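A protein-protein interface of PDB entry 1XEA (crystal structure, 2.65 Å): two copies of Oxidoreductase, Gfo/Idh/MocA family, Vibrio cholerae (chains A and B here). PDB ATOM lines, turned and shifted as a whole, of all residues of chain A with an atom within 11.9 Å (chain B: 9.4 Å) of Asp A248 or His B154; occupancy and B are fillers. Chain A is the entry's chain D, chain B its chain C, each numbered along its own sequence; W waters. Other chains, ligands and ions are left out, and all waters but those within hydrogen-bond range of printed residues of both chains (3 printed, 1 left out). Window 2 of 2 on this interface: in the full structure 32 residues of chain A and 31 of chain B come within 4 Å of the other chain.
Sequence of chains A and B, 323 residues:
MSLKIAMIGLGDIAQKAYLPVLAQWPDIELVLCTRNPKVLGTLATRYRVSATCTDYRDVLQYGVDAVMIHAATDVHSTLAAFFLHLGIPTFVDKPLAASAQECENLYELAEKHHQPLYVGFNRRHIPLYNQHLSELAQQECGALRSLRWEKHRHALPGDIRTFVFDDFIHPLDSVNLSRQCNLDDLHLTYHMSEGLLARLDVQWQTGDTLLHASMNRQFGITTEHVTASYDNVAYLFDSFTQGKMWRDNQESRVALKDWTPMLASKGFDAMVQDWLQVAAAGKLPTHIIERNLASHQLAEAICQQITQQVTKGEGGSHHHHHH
N of Ala B155 lies close to OD1 of Asn A232, 3.1 Å away. The side-chain amide nitrogen of Asn B216 is in hydrogen-bond range of the side-chain hydroxyl of Ser A229, at 3.5 Å. The backbone carbonyl oxygen (O) of Gln B218 is in hydrogen-bond range of the backbone NH (N) of Asn A232 (2.7 Å). O of Gly B220 sits at hydrogen-bond distance from N of Arg A247 (3.2 Å). O of Gly B220 is in hydrogen-bond range of N of Asn A249 (3.2 Å). The side-chain amide nitrogen of Asn A249 sits close to the backbone NH of Thr B222 (2.6 Å). The backbone carbonyl oxygen of Gln B218 sits close to the backbone carbonyl oxygen of Tyr A230 (3.5 Å).
N of Arg B153 sits at hydrogen-bond distance from O of Asn B216 (3.0 Å). The backbone carbonyl oxygen (O) of Arg B153 is in hydrogen-bond range of the backbone NH (N) of Gln B218, 3.5 Å away. N of Phe B219 lies within hydrogen-bond range of O of Arg B153 (2.9 Å). The side-chain amide oxygen (OD1) of Asn B216 sits at hydrogen-bond distance from the backbone NH (N) of Gln B218 (2.8 Å). The side-chain amide oxygen (OD1) of Asn B216 sits at hydrogen-bond distance from the backbone NH (N) of Phe B219. The backbone carbonyl oxygen of Ala A234 sits at hydrogen-bond distance from the backbone NH of Trp A246, at 2.8 Å.
Ser A229 touches Phe B219. C of Asp A231 touches O of Gln B218 (3.7 Å). CA of Asn A232 touches O of Phe B219, 3.7 Å away. Val A233 touches Gly B220 (N to CA, 3.6 Å). CE1 of Phe B219 touches CB of Ala A234 (3.5 Å). N of Ala A234 touches CA of Gly B220 (3.9 Å). Trp A246 touches Ile B221 (CG to CG2, 3.4 Å). His B154 touches Asp A248 (NE2 to CA, 3.6 Å). Asn A249 touches Ile B221. CD1 of Ile B221 touches C of Gln A250, 3.9 Å away.
Of the printed residues of chain B, Asp A231 touches Gln B218. Of the printed residues of chain B, Val A233 touches Gly B220. Of the printed residues of chain B, Ala A234 touches Phe B219 (3.5 Å) and Gly B220 (3.9 Å). Printed residues of chain B within 4 Å of Asp A248: His B154 and Gly B220. Gln A250 touches one residue of chain B. His B154 touches just these residues of chain A: Asp A248 and Asn A249. Ala B155 touches one residue of chain A. No residue of chain A comes within 4 Å of Leu B156. Met B215 touches none of the printed residues of chain A. Printed residues of chain A within 4 Å of Asn B216: Ser A229 (3.5 Å). Ile B221 touches just these residues of chain A: Trp A246 (3.4 Å), Asn A249 (3.1 Å) and Gln A250 (3.9 Å).
Hydrophobic or aromatic side chains of chain B that line the printed part of chain A: His B154, Ala B155, Phe B219 and Ile B221. Hydrophobic or aromatic side chains of chain A within 4 Å of the printed part of chain B: Ala A234 and Trp A246.
No position is printed for both chains. Of the 22 pairs that touch across the chains among the printed residues, none has its exchanged pair printed and touching as well.
Water W1 lies within hydrogen-bond range of the side-chain amide nitrogen of Gln B218 (2.5 Å) and the side-chain amide nitrogen of Asn A232 (3.3 Å). Water W2 lies within hydrogen-bond range of OD1 of Asn A249 (2.8 Å) and OG1 of Thr B222 (3.0 Å). Water W3 lies within hydrogen-bond range of O of Thr B222 (3.0 Å) and ND2 of Asn A249 (3.5 Å).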
ATOM      1  N   SER A 229      -1.575  36.368 -22.768  1.00  0.00           N
ATOM      2  CA  SER A 229      -1.255  34.983 -22.468  1.00  0.00           C
ATOM      3  C   SER A 229      -0.721  34.781 -21.068  1.00  0.00           C
ATOM      4  O   SER A 229      -0.027  35.631 -20.525  1.00  0.00           O
ATOM      5  CB  SER A 229      -0.242  34.441 -23.463  1.00  0.00           C
ATOM      6  OG  SER A 229       1.046  34.953 -23.182  1.00  0.00           O
ATOM      7  N   TYR A 230      -1.072  33.644 -20.486  1.00  0.00           N
ATOM      8  CA  TYR A 230      -0.603  33.268 -19.163  1.00  0.00           C
ATOM      9  C   TYR A 230       0.224  32.007 -19.385  1.00  0.00           C
ATOM     10  O   TYR A 230       0.775  31.786 -20.471  1.00  0.00           O
ATOM     11  CB  TYR A 230      -1.781  32.956 -18.250  1.00  0.00           C
ATOM     12  CG  TYR A 230      -2.745  34.106 -18.085  1.00  0.00           C
ATOM     13  CD1 TYR A 230      -3.800  34.288 -18.984  1.00  0.00           C
ATOM     14  CD2 TYR A 230      -2.598  35.024 -17.034  1.00  0.00           C
ATOM     15  CE1 TYR A 230      -4.683  35.344 -18.844  1.00  0.00           C
ATOM     16  CE2 TYR A 230      -3.480  36.093 -16.885  1.00  0.00           C
ATOM     17  CZ  TYR A 230      -4.518  36.242 -17.798  1.00  0.00           C
ATOM     18  OH  TYR A 230      -5.394  37.290 -17.680  1.00  0.00           O
ATOM     19  N   ASP A 231       0.311  31.160 -18.379  1.00  0.00           N
ATOM     20  CA  ASP A 231       1.071  29.950 -18.582  1.00  0.00           C
ATOM     21  C   ASP A 231       0.126  28.890 -19.116  1.00  0.00           C
ATOM     22  O   ASP A 231      -0.824  28.487 -18.447  1.00  0.00           O
ATOM     23  CB  ASP A 231       1.747  29.500 -17.273  1.00  0.00           C
ATOM     24  CG  ASP A 231       2.917  30.410 -16.870  1.00  0.00           C
ATOM     25  OD1 ASP A 231       3.607  30.923 -17.788  1.00  0.00           O
ATOM     26  OD2 ASP A 231       3.158  30.602 -15.651  1.00  0.00           O
ATOM     27  N   ASN A 232       0.372  28.465 -20.345  1.00  0.00           N
ATOM     28  CA  ASN A 232      -0.462  27.446 -20.966  1.00  0.00           C
ATOM     29  C   ASN A 232      -1.910  27.878 -21.243  1.00  0.00           C
ATOM     30  O   ASN A 232      -2.792  27.053 -21.520  1.00  0.00           O
ATOM     31  CB  ASN A 232      -0.432  26.188 -20.110  1.00  0.00           C
ATOM     32  CG  ASN A 232       0.975  25.630 -19.966  1.00  0.00           C
ATOM     33  OD1 ASN A 232       1.741  25.601 -20.940  1.00  0.00           O
ATOM     34  ND2 ASN A 232       1.322  25.173 -18.763  1.00  0.00           N
ATOM     35  N   VAL A 233      -2.149  29.183 -21.188  1.00  0.00           N
ATOM     36  CA  VAL A 233      -3.470  29.725 -21.453  1.00  0.00           C
ATOM     37  C   VAL A 233      -3.315  31.050 -22.189  1.00  0.00           C
ATOM     38  O   VAL A 233      -2.393  31.811 -21.900  1.00  0.00           O
ATOM     39  CB  VAL A 233      -4.258  29.967 -20.136  1.00  0.00           C
ATOM     40  CG1 VAL A 233      -5.646  30.515 -20.448  1.00  0.00           C
ATOM     41  CG2 VAL A 233      -4.374  28.677 -19.345  1.00  0.00           C
ATOM     42  N   ALA A 234      -4.210  31.326 -23.136  1.00  0.00           N
ATOM     43  CA  ALA A 234      -4.155  32.581 -23.893  1.00  0.00           C
ATOM     44  C   ALA A 234      -5.504  32.978 -24.468  1.00  0.00           C
ATOM     45  O   ALA A 234      -6.387  32.143 -24.658  1.00  0.00           O
ATOM     46  CB  ALA A 234      -3.135  32.465 -25.021  1.00  0.00           C
ATOM     47  N   TYR A 235      -5.667  34.267 -24.722  1.00  0.00           N
ATOM     48  CA  TYR A 235      -6.904  34.760 -25.298  1.00  0.00           C
ATOM     49  C   TYR A 235      -6.565  35.710 -26.415  1.00  0.00           C
ATOM     50  O   TYR A 235      -5.514  36.347 -26.405  1.00  0.00           O
ATOM     51  CB  TYR A 235      -7.742  35.520 -24.272  1.00  0.00           C
ATOM     52  CG  TYR A 235      -8.180  34.723 -23.065  1.00  0.00           C
ATOM     53  CD1 TYR A 235      -7.266  34.359 -22.067  1.00  0.00           C
ATOM     54  CD2 TYR A 235      -9.519  34.382 -22.889  1.00  0.00           C
ATOM     55  CE1 TYR A 235      -7.685  33.678 -20.916  1.00  0.00           C
ATOM     56  CE2 TYR A 235      -9.948  33.709 -21.754  1.00  0.00           C
ATOM     57  CZ  TYR A 235      -9.035  33.362 -20.772  1.00  0.00           C
ATOM     58  OH  TYR A 235      -9.479  32.722 -19.642  1.00  0.00           O
ATOM     59  N   LYS A 244     -11.299  34.384 -28.621  1.00  0.00           N
ATOM     60  CA  LYS A 244     -10.963  32.967 -28.615  1.00  0.00           C
ATOM     61  C   LYS A 244     -10.138  32.656 -27.393  1.00  0.00           C
ATOM     62  O   LYS A 244      -9.219  33.392 -27.053  1.00  0.00           O
ATOM     63  CB  LYS A 244     -10.180  32.562 -29.871  1.00  0.00           C
ATOM     64  CG  LYS A 244     -10.962  32.773 -31.145  1.00  0.00           C
ATOM     65  CD  LYS A 244     -10.370  32.023 -32.305  1.00  0.00           C
ATOM     66  CE  LYS A 244      -9.487  32.887 -33.162  1.00  0.00           C
ATOM     67  NZ  LYS A 244      -9.327  32.250 -34.506  1.00  0.00           N
ATOM     68  N   MET A 245     -10.494  31.578 -26.712  1.00  0.00           N
ATOM     69  CA  MET A 245      -9.751  31.163 -25.543  1.00  0.00           C
ATOM     70  C   MET A 245      -9.010  29.881 -25.892  1.00  0.00           C
ATOM     71  O   MET A 245      -9.591  28.926 -26.415  1.00  0.00           O
ATOM     72  CB  MET A 245     -10.675  30.923 -24.359  1.00  0.00           C
ATOM     73  CG  MET A 245      -9.929  30.575 -23.083  1.00  0.00           C
ATOM     74  SD  MET A 245     -11.145  30.183 -21.620  1.00  0.00           S
ATOM     75  CE  MET A 245     -11.579  28.355 -22.173  1.00  0.00           C
ATOM     76  N   TRP A 246      -7.716  29.881 -25.604  1.00  0.00           N
ATOM     77  CA  TRP A 246      -6.855  28.749 -25.872  1.00  0.00           C
ATOM     78  C   TRP A 246      -6.321  28.151 -24.575  1.00  0.00           C
ATOM     79  O   TRP A 246      -5.684  28.836 -23.776  1.00  0.00           O
ATOM     80  CB  TRP A 246      -5.683  29.200 -26.744  1.00  0.00           C
ATOM     81  CG  TRP A 246      -6.050  29.562 -28.156  1.00  0.00           C
ATOM     82  CD1 TRP A 246      -6.738  28.790 -29.043  1.00  0.00           C
ATOM     83  CD2 TRP A 246      -5.652  30.740 -28.881  1.00  0.00           C
ATOM     84  NE1 TRP A 246      -6.791  29.404 -30.274  1.00  0.00           N
ATOM     85  CE2 TRP A 246      -6.134  30.603 -30.201  1.00  0.00           C
ATOM     86  CE3 TRP A 246      -4.937  31.897 -28.542  1.00  0.00           C
ATOM     87  CZ2 TRP A 246      -5.918  31.571 -31.185  1.00  0.00           C
ATOM     88  CZ3 TRP A 246      -4.722  32.865 -29.527  1.00  0.00           C
ATOM     89  CH2 TRP A 246      -5.215  32.693 -30.830  1.00  0.00           C
ATOM     90  N   ARG A 247      -6.605  26.877 -24.357  1.00  0.00           N
ATOM     91  CA  ARG A 247      -6.103  26.179 -23.178  1.00  0.00           C
ATOM     92  C   ARG A 247      -6.231  24.689 -23.413  1.00  0.00           C
ATOM     93  O   ARG A 247      -7.178  24.238 -24.048  1.00  0.00           O
ATOM     94  CB  ARG A 247      -6.869  26.587 -21.916  1.00  0.00           C
ATOM     95  CG  ARG A 247      -8.332  26.238 -21.899  1.00  0.00           C
ATOM     96  CD  ARG A 247      -8.881  26.462 -20.503  1.00  0.00           C
ATOM     97  NE  ARG A 247      -8.318  27.668 -19.895  1.00  0.00           N
ATOM     98  CZ  ARG A 247      -8.889  28.339 -18.899  1.00  0.00           C
ATOM     99  NH1 ARG A 247     -10.044  27.914 -18.409  1.00  0.00           N
ATOM    100  NH2 ARG A 247      -8.314  29.427 -18.389  1.00  0.00           N
ATOM    101  N   ASP A 248      -5.273  23.921 -22.924  1.00  0.00           N
ATOM    102  CA  ASP A 248      -5.330  22.485 -23.124  1.00  0.00           C
ATOM    103  C   ASP A 248      -5.209  22.164 -24.615  1.00  0.00           C
ATOM    104  O   ASP A 248      -5.661  21.117 -25.068  1.00  0.00           O
ATOM    105  CB  ASP A 248      -6.654  21.922 -22.579  1.00  0.00           C
ATOM    106  CG  ASP A 248      -6.833  22.177 -21.089  1.00  0.00           C
ATOM    107  OD1 ASP A 248      -5.935  21.770 -20.312  1.00  0.00           O
ATOM    108  OD2 ASP A 248      -7.868  22.781 -20.688  1.00  0.00           O
ATOM    109  N   ASN A 249      -4.583  23.063 -25.369  1.00  0.00           N
ATOM    110  CA  ASN A 249      -4.408  22.900 -26.818  1.00  0.00           C
ATOM    111  C   ASN A 249      -5.754  22.827 -27.557  1.00  0.00           C
ATOM    112  O   ASN A 249      -5.842  22.273 -28.651  1.00  0.00           O
ATOM    113  CB  ASN A 249      -3.567  21.651 -27.146  1.00  0.00           C
ATOM    114  CG  ASN A 249      -2.603  21.874 -28.323  1.00  0.00           C
ATOM    115  OD1 ASN A 249      -2.116  20.925 -28.928  1.00  0.00           O
ATOM    116  ND2 ASN A 249      -2.316  23.130 -28.629  1.00  0.00           N
ATOM    117  N   GLN A 250      -6.797  23.377 -26.952  1.00  0.00           N
ATOM    118  CA  GLN A 250      -8.098  23.411 -27.584  1.00  0.00           C
ATOM    119  C   GLN A 250      -8.489  24.876 -27.698  1.00  0.00           C
ATOM    120  O   GLN A 250      -8.060  25.703 -26.888  1.00  0.00           O
ATOM    121  CB  GLN A 250      -9.133  22.684 -26.746  1.00  0.00           C
ATOM    122  CG  GLN A 250      -8.867  21.212 -26.597  1.00  0.00           C
ATOM    123  CD  GLN A 250      -9.624  20.602 -25.425  1.00  0.00           C
ATOM    124  OE1 GLN A 250      -9.536  19.401 -25.179  1.00  0.00           O
ATOM    125  NE2 GLN A 250     -10.367  21.431 -24.693  1.00  0.00           N
ATOM    126  N   GLU A 251      -9.303  25.189 -28.702  1.00  0.00           N
ATOM    127  CA  GLU A 251      -9.766  26.547 -28.941  1.00  0.00           C
ATOM    128  C   GLU A 251     -11.278  26.620 -28.859  1.00  0.00           C
ATOM    129  O   GLU A 251     -11.980  25.803 -29.449  1.00  0.00           O
ATOM    130  CB  GLU A 251      -9.316  27.022 -30.324  1.00  0.00           C
ATOM    131  CG  GLU A 251     -10.074  28.240 -30.841  1.00  0.00           C
ATOM    132  CD  GLU A 251      -9.492  28.776 -32.117  1.00  0.00           C
ATOM    133  OE1 GLU A 251     -10.267  29.141 -33.041  1.00  0.00           O
ATOM    134  OE2 GLU A 251      -8.248  28.844 -32.199  1.00  0.00           O
ATOM    135  N   SER A 252     -11.770  27.607 -28.121  1.00  0.00           N
ATOM    136  CA  SER A 252     -13.203  27.824 -27.968  1.00  0.00           C
ATOM    137  C   SER A 252     -13.446  29.325 -28.028  1.00  0.00           C
ATOM    138  O   SER A 252     -12.517  30.116 -27.840  1.00  0.00           O
ATOM    139  CB  SER A 252     -13.677  27.278 -26.627  1.00  0.00           C
ATOM    140  OG  SER A 252     -12.986  27.906 -25.568  1.00  0.00           O
ATOM    141  N   LYS B 151       5.433  31.461 -33.451  1.00  0.00           N
ATOM    142  CA  LYS B 151       5.336  30.011 -33.497  1.00  0.00           C
ATOM    143  C   LYS B 151       5.209  29.576 -32.048  1.00  0.00           C
ATOM    144  O   LYS B 151       6.203  29.521 -31.333  1.00  0.00           O
ATOM    145  CB  LYS B 151       6.594  29.419 -34.134  1.00  0.00           C
ATOM    146  CG  LYS B 151       6.405  28.001 -34.655  1.00  0.00           C
ATOM    147  CD  LYS B 151       7.688  27.431 -35.261  1.00  0.00           C
ATOM    148  CE  LYS B 151       7.450  26.029 -35.749  1.00  0.00           C
ATOM    149  NZ  LYS B 151       6.795  25.202 -34.702  1.00  0.00           N
ATOM    150  N   HIS B 152       3.984  29.286 -31.614  1.00  0.00           N
ATOM    151  CA  HIS B 152       3.756  28.891 -30.234  1.00  0.00           C
ATOM    152  C   HIS B 152       3.476  27.408 -30.088  1.00  0.00           C
ATOM    153  O   HIS B 152       3.115  26.735 -31.056  1.00  0.00           O
ATOM    154  CB  HIS B 152       2.599  29.688 -29.625  1.00  0.00           C
ATOM    155  CG  HIS B 152       2.720  31.170 -29.810  1.00  0.00           C
ATOM    156  ND1 HIS B 152       3.904  31.787 -30.151  1.00  0.00           N
ATOM    157  CD2 HIS B 152       1.801  32.157 -29.702  1.00  0.00           C
ATOM    158  CE1 HIS B 152       3.710  33.091 -30.249  1.00  0.00           C
ATOM    159  NE2 HIS B 152       2.442  33.341 -29.980  1.00  0.00           N
ATOM    160  N   ARG B 153       3.670  26.907 -28.868  1.00  0.00           N
ATOM    161  CA  ARG B 153       3.437  25.504 -28.532  1.00  0.00           C
ATOM    162  C   ARG B 153       2.742  25.441 -27.192  1.00  0.00           C
ATOM    163  O   ARG B 153       2.872  26.341 -26.368  1.00  0.00           O
ATOM    164  CB  ARG B 153       4.750  24.716 -28.440  1.00  0.00           C
ATOM    165  CG  ARG B 153       5.518  24.591 -29.749  1.00  0.00           C
ATOM    166  CD  ARG B 153       6.477  23.405 -29.728  1.00  0.00           C
ATOM    167  NE  ARG B 153       6.276  22.555 -30.900  1.00  0.00           N
ATOM    168  CZ  ARG B 153       6.860  22.747 -32.076  1.00  0.00           C
ATOM    169  NH1 ARG B 153       7.702  23.758 -32.253  1.00  0.00           N
ATOM    170  NH2 ARG B 153       6.576  21.938 -33.089  1.00  0.00           N
ATOM    171  N   HIS B 154       1.997  24.373 -26.973  1.00  0.00           N
ATOM    172  CA  HIS B 154       1.298  24.220 -25.715  1.00  0.00           C
ATOM    173  C   HIS B 154       2.159  23.436 -24.723  1.00  0.00           C
ATOM    174  O   HIS B 154       2.795  22.446 -25.089  1.00  0.00           O
ATOM    175  CB  HIS B 154      -0.029  23.506 -25.950  1.00  0.00           C
ATOM    176  CG  HIS B 154      -0.721  23.093 -24.691  1.00  0.00           C
ATOM    177  ND1 HIS B 154      -0.972  23.973 -23.663  1.00  0.00           N
ATOM    178  CD2 HIS B 154      -1.244  21.905 -24.307  1.00  0.00           C
ATOM    179  CE1 HIS B 154      -1.626  23.346 -22.700  1.00  0.00           C
ATOM    180  NE2 HIS B 154      -1.802  22.091 -23.066  1.00  0.00           N
ATOM    181  N   ALA B 155       2.191  23.918 -23.481  1.00  0.00           N
ATOM    182  CA  ALA B 155       2.929  23.295 -22.383  1.00  0.00           C
ATOM    183  C   ALA B 155       4.205  22.534 -22.786  1.00  0.00           C
ATOM    184  O   ALA B 155       4.330  21.341 -22.510  1.00  0.00           O
ATOM    185  CB  ALA B 155       1.989  22.369 -21.645  1.00  0.00           C
ATOM    186  N   LEU B 156       5.165  23.214 -23.401  1.00  0.00           N
ATOM    187  CA  LEU B 156       6.372  22.530 -23.829  1.00  0.00           C
ATOM    188  C   LEU B 156       7.658  23.345 -23.667  1.00  0.00           C
ATOM    189  O   LEU B 156       8.352  23.624 -24.646  1.00  0.00           O
ATOM    190  CB  LEU B 156       6.221  22.121 -25.294  1.00  0.00           C
ATOM    191  CG  LEU B 156       7.161  21.032 -25.810  1.00  0.00           C
ATOM    192  CD1 LEU B 156       6.460  19.694 -25.687  1.00  0.00           C
ATOM    193  CD2 LEU B 156       7.536  21.309 -27.260  1.00  0.00           C
ATOM    194  N   PRO B 157       7.998  23.727 -22.429  1.00  0.00           N
ATOM    195  CA  PRO B 157       9.214  24.509 -22.175  1.00  0.00           C
ATOM    196  C   PRO B 157      10.460  23.650 -22.357  1.00  0.00           C
ATOM    197  O   PRO B 157      10.384  22.426 -22.260  1.00  0.00           O
ATOM    198  CB  PRO B 157       9.023  24.973 -20.740  1.00  0.00           C
ATOM    199  CG  PRO B 157       8.326  23.795 -20.129  1.00  0.00           C
ATOM    200  CD  PRO B 157       7.297  23.413 -21.172  1.00  0.00           C
ATOM    201  N   GLY B 158      11.599  24.287 -22.616  1.00  0.00           N
ATOM    202  CA  GLY B 158      12.828  23.540 -22.814  1.00  0.00           C
ATOM    203  C   GLY B 158      14.065  24.348 -22.485  1.00  0.00           C
ATOM    204  O   GLY B 158      13.967  25.522 -22.144  1.00  0.00           O
ATOM    205  N   ASP B 167      14.264  25.206 -32.470  1.00  0.00           N
ATOM    206  CA  ASP B 167      12.887  25.645 -32.663  1.00  0.00           C
ATOM    207  C   ASP B 167      12.792  27.108 -33.102  1.00  0.00           C
ATOM    208  O   ASP B 167      12.367  27.411 -34.219  1.00  0.00           O
ATOM    209  CB  ASP B 167      12.118  25.455 -31.354  1.00  0.00           C
ATOM    210  CG  ASP B 167      10.702  24.962 -31.567  1.00  0.00           C
ATOM    211  OD1 ASP B 167      10.206  25.028 -32.710  1.00  0.00           O
ATOM    212  OD2 ASP B 167      10.070  24.515 -30.582  1.00  0.00           O
ATOM    213  N   ALA B 198      10.572  29.434 -21.419  1.00  0.00           N
ATOM    214  CA  ALA B 198       9.148  29.334 -21.745  1.00  0.00           C
ATOM    215  C   ALA B 198       8.806  30.100 -23.025  1.00  0.00           C
ATOM    216  O   ALA B 198       8.295  29.511 -23.980  1.00  0.00           O
ATOM    217  CB  ALA B 198       8.309  29.846 -20.580  1.00  0.00           C
ATOM    218  N   MET B 215       8.084  33.355 -29.923  1.00  0.00           N
ATOM    219  CA  MET B 215       7.838  31.942 -29.663  1.00  0.00           C
ATOM    220  C   MET B 215       7.467  31.720 -28.219  1.00  0.00           C
ATOM    221  O   MET B 215       8.288  31.923 -27.331  1.00  0.00           O
ATOM    222  CB  MET B 215       9.071  31.109 -29.968  1.00  0.00           C
ATOM    223  CG  MET B 215       8.877  29.645 -29.675  1.00  0.00           C
ATOM    224  SD  MET B 215      10.213  28.547 -30.528  1.00  0.00           S
ATOM    225  CE  MET B 215      10.611  27.414 -29.034  1.00  0.00           C
ATOM    226  N   ASN B 216       6.231  31.302 -27.977  1.00  0.00           N
ATOM    227  CA  ASN B 216       5.799  31.036 -26.616  1.00  0.00           C
ATOM    228  C   ASN B 216       5.524  29.548 -26.505  1.00  0.00           C
ATOM    229  O   ASN B 216       4.472  29.059 -26.925  1.00  0.00           O
ATOM    230  CB  ASN B 216       4.543  31.832 -26.271  1.00  0.00           C
ATOM    231  CG  ASN B 216       4.205  31.776 -24.789  1.00  0.00           C
ATOM    232  OD1 ASN B 216       4.458  30.772 -24.116  1.00  0.00           O
ATOM    233  ND2 ASN B 216       3.616  32.845 -24.277  1.00  0.00           N
ATOM    234  N   ARG B 217       6.491  28.835 -25.939  1.00  0.00           N
ATOM    235  CA  ARG B 217       6.392  27.394 -25.759  1.00  0.00           C
ATOM    236  C   ARG B 217       5.536  27.025 -24.564  1.00  0.00           C
ATOM    237  O   ARG B 217       5.504  25.873 -24.142  1.00  0.00           O
ATOM    238  CB  ARG B 217       7.785  26.787 -25.614  1.00  0.00           C
ATOM    239  CG  ARG B 217       8.563  26.777 -26.914  1.00  0.00           C
ATOM    240  CD  ARG B 217       8.257  25.552 -27.735  1.00  0.00           C
ATOM    241  NE  ARG B 217       8.766  24.347 -27.087  1.00  0.00           N
ATOM    242  CZ  ARG B 217      10.029  23.941 -27.146  1.00  0.00           C
ATOM    243  NH1 ARG B 217      10.933  24.630 -27.834  1.00  0.00           N
ATOM    244  NH2 ARG B 217      10.387  22.847 -26.500  1.00  0.00           N
ATOM    245  N   GLN B 218       4.845  28.012 -24.011  1.00  0.00           N
ATOM    246  CA  GLN B 218       3.964  27.749 -22.893  1.00  0.00           C
ATOM    247  C   GLN B 218       2.678  28.504 -23.157  1.00  0.00           C
ATOM    248  O   GLN B 218       2.088  29.107 -22.261  1.00  0.00           O
ATOM    249  CB  GLN B 218       4.611  28.194 -21.591  1.00  0.00           C
ATOM    250  CG  GLN B 218       4.231  27.331 -20.412  1.00  0.00           C
ATOM    251  CD  GLN B 218       5.396  27.097 -19.457  1.00  0.00           C
ATOM    252  OE1 GLN B 218       5.868  28.019 -18.786  1.00  0.00           O
ATOM    253  NE2 GLN B 218       5.864  25.854 -19.393  1.00  0.00           N
ATOM    254  N   PHE B 219       2.257  28.447 -24.421  1.00  0.00           N
ATOM    255  CA  PHE B 219       1.042  29.103 -24.923  1.00  0.00           C
ATOM    256  C   PHE B 219      -0.191  28.206 -24.720  1.00  0.00           C
ATOM    257  O   PHE B 219      -0.070  26.989 -24.569  1.00  0.00           O
ATOM    258  CB  PHE B 219       1.217  29.394 -26.419  1.00  0.00           C
ATOM    259  CG  PHE B 219       0.319  30.482 -26.955  1.00  0.00           C
ATOM    260  CD1 PHE B 219       0.455  31.802 -26.516  1.00  0.00           C
ATOM    261  CD2 PHE B 219      -0.595  30.212 -27.965  1.00  0.00           C
ATOM    262  CE1 PHE B 219      -0.285  32.831 -27.085  1.00  0.00           C
ATOM    263  CE2 PHE B 219      -1.337  31.234 -28.537  1.00  0.00           C
ATOM    264  CZ  PHE B 219      -1.180  32.551 -28.093  1.00  0.00           C
ATOM    265  N   GLY B 220      -1.373  28.807 -24.743  1.00  0.00           N
ATOM    266  CA  GLY B 220      -2.586  28.034 -24.570  1.00  0.00           C
ATOM    267  C   GLY B 220      -2.872  27.030 -25.678  1.00  0.00           C
ATOM    268  O   GLY B 220      -3.736  26.167 -25.527  1.00  0.00           O
ATOM    269  N   ILE B 221      -2.153  27.121 -26.795  1.00  0.00           N
ATOM    270  CA  ILE B 221      -2.375  26.198 -27.915  1.00  0.00           C
ATOM    271  C   ILE B 221      -1.199  26.211 -28.895  1.00  0.00           C
ATOM    272  O   ILE B 221      -0.494  27.210 -29.017  1.00  0.00           O
ATOM    273  CB  ILE B 221      -3.678  26.565 -28.700  1.00  0.00           C
ATOM    274  CG1 ILE B 221      -4.077  25.417 -29.628  1.00  0.00           C
ATOM    275  CG2 ILE B 221      -3.449  27.838 -29.527  1.00  0.00           C
ATOM    276  CD1 ILE B 221      -5.496  25.504 -30.159  1.00  0.00           C
ATOM    277  N   THR B 222      -0.976  25.096 -29.582  1.00  0.00           N
ATOM    278  CA  THR B 222       0.106  25.029 -30.553  1.00  0.00           C
ATOM    279  C   THR B 222      -0.431  25.638 -31.860  1.00  0.00           C
ATOM    280  O   THR B 222      -1.441  25.184 -32.396  1.00  0.00           O
ATOM    281  CB  THR B 222       0.568  23.557 -30.757  1.00  0.00           C
ATOM    282  OG1 THR B 222       0.989  23.024 -29.495  1.00  0.00           O
ATOM    283  CG2 THR B 222       1.735  23.471 -31.730  1.00  0.00           C
ATOM    284  N   THR B 223       0.226  26.690 -32.343  1.00  0.00           N
ATOM    285  CA  THR B 223      -0.188  27.367 -33.566  1.00  0.00           C
ATOM    286  C   THR B 223       0.935  28.272 -34.095  1.00  0.00           C
ATOM    287  O   THR B 223       1.885  28.606 -33.374  1.00  0.00           O
ATOM    288  CB  THR B 223      -1.494  28.218 -33.335  1.00  0.00           C
ATOM    289  OG1 THR B 223      -1.918  28.794 -34.579  1.00  0.00           O
ATOM    290  CG2 THR B 223      -1.251  29.350 -32.318  1.00  0.00           C
HETATM  291  O   HOH W   1       4.381  23.956 -18.883  1.00  0.00           O
HETATM  292  O   HOH W   2       0.347  20.090 -30.018  1.00  0.00           O
HETATM  293  O   HOH W   3      -3.043  22.673 -31.978  1.00  0.00           O
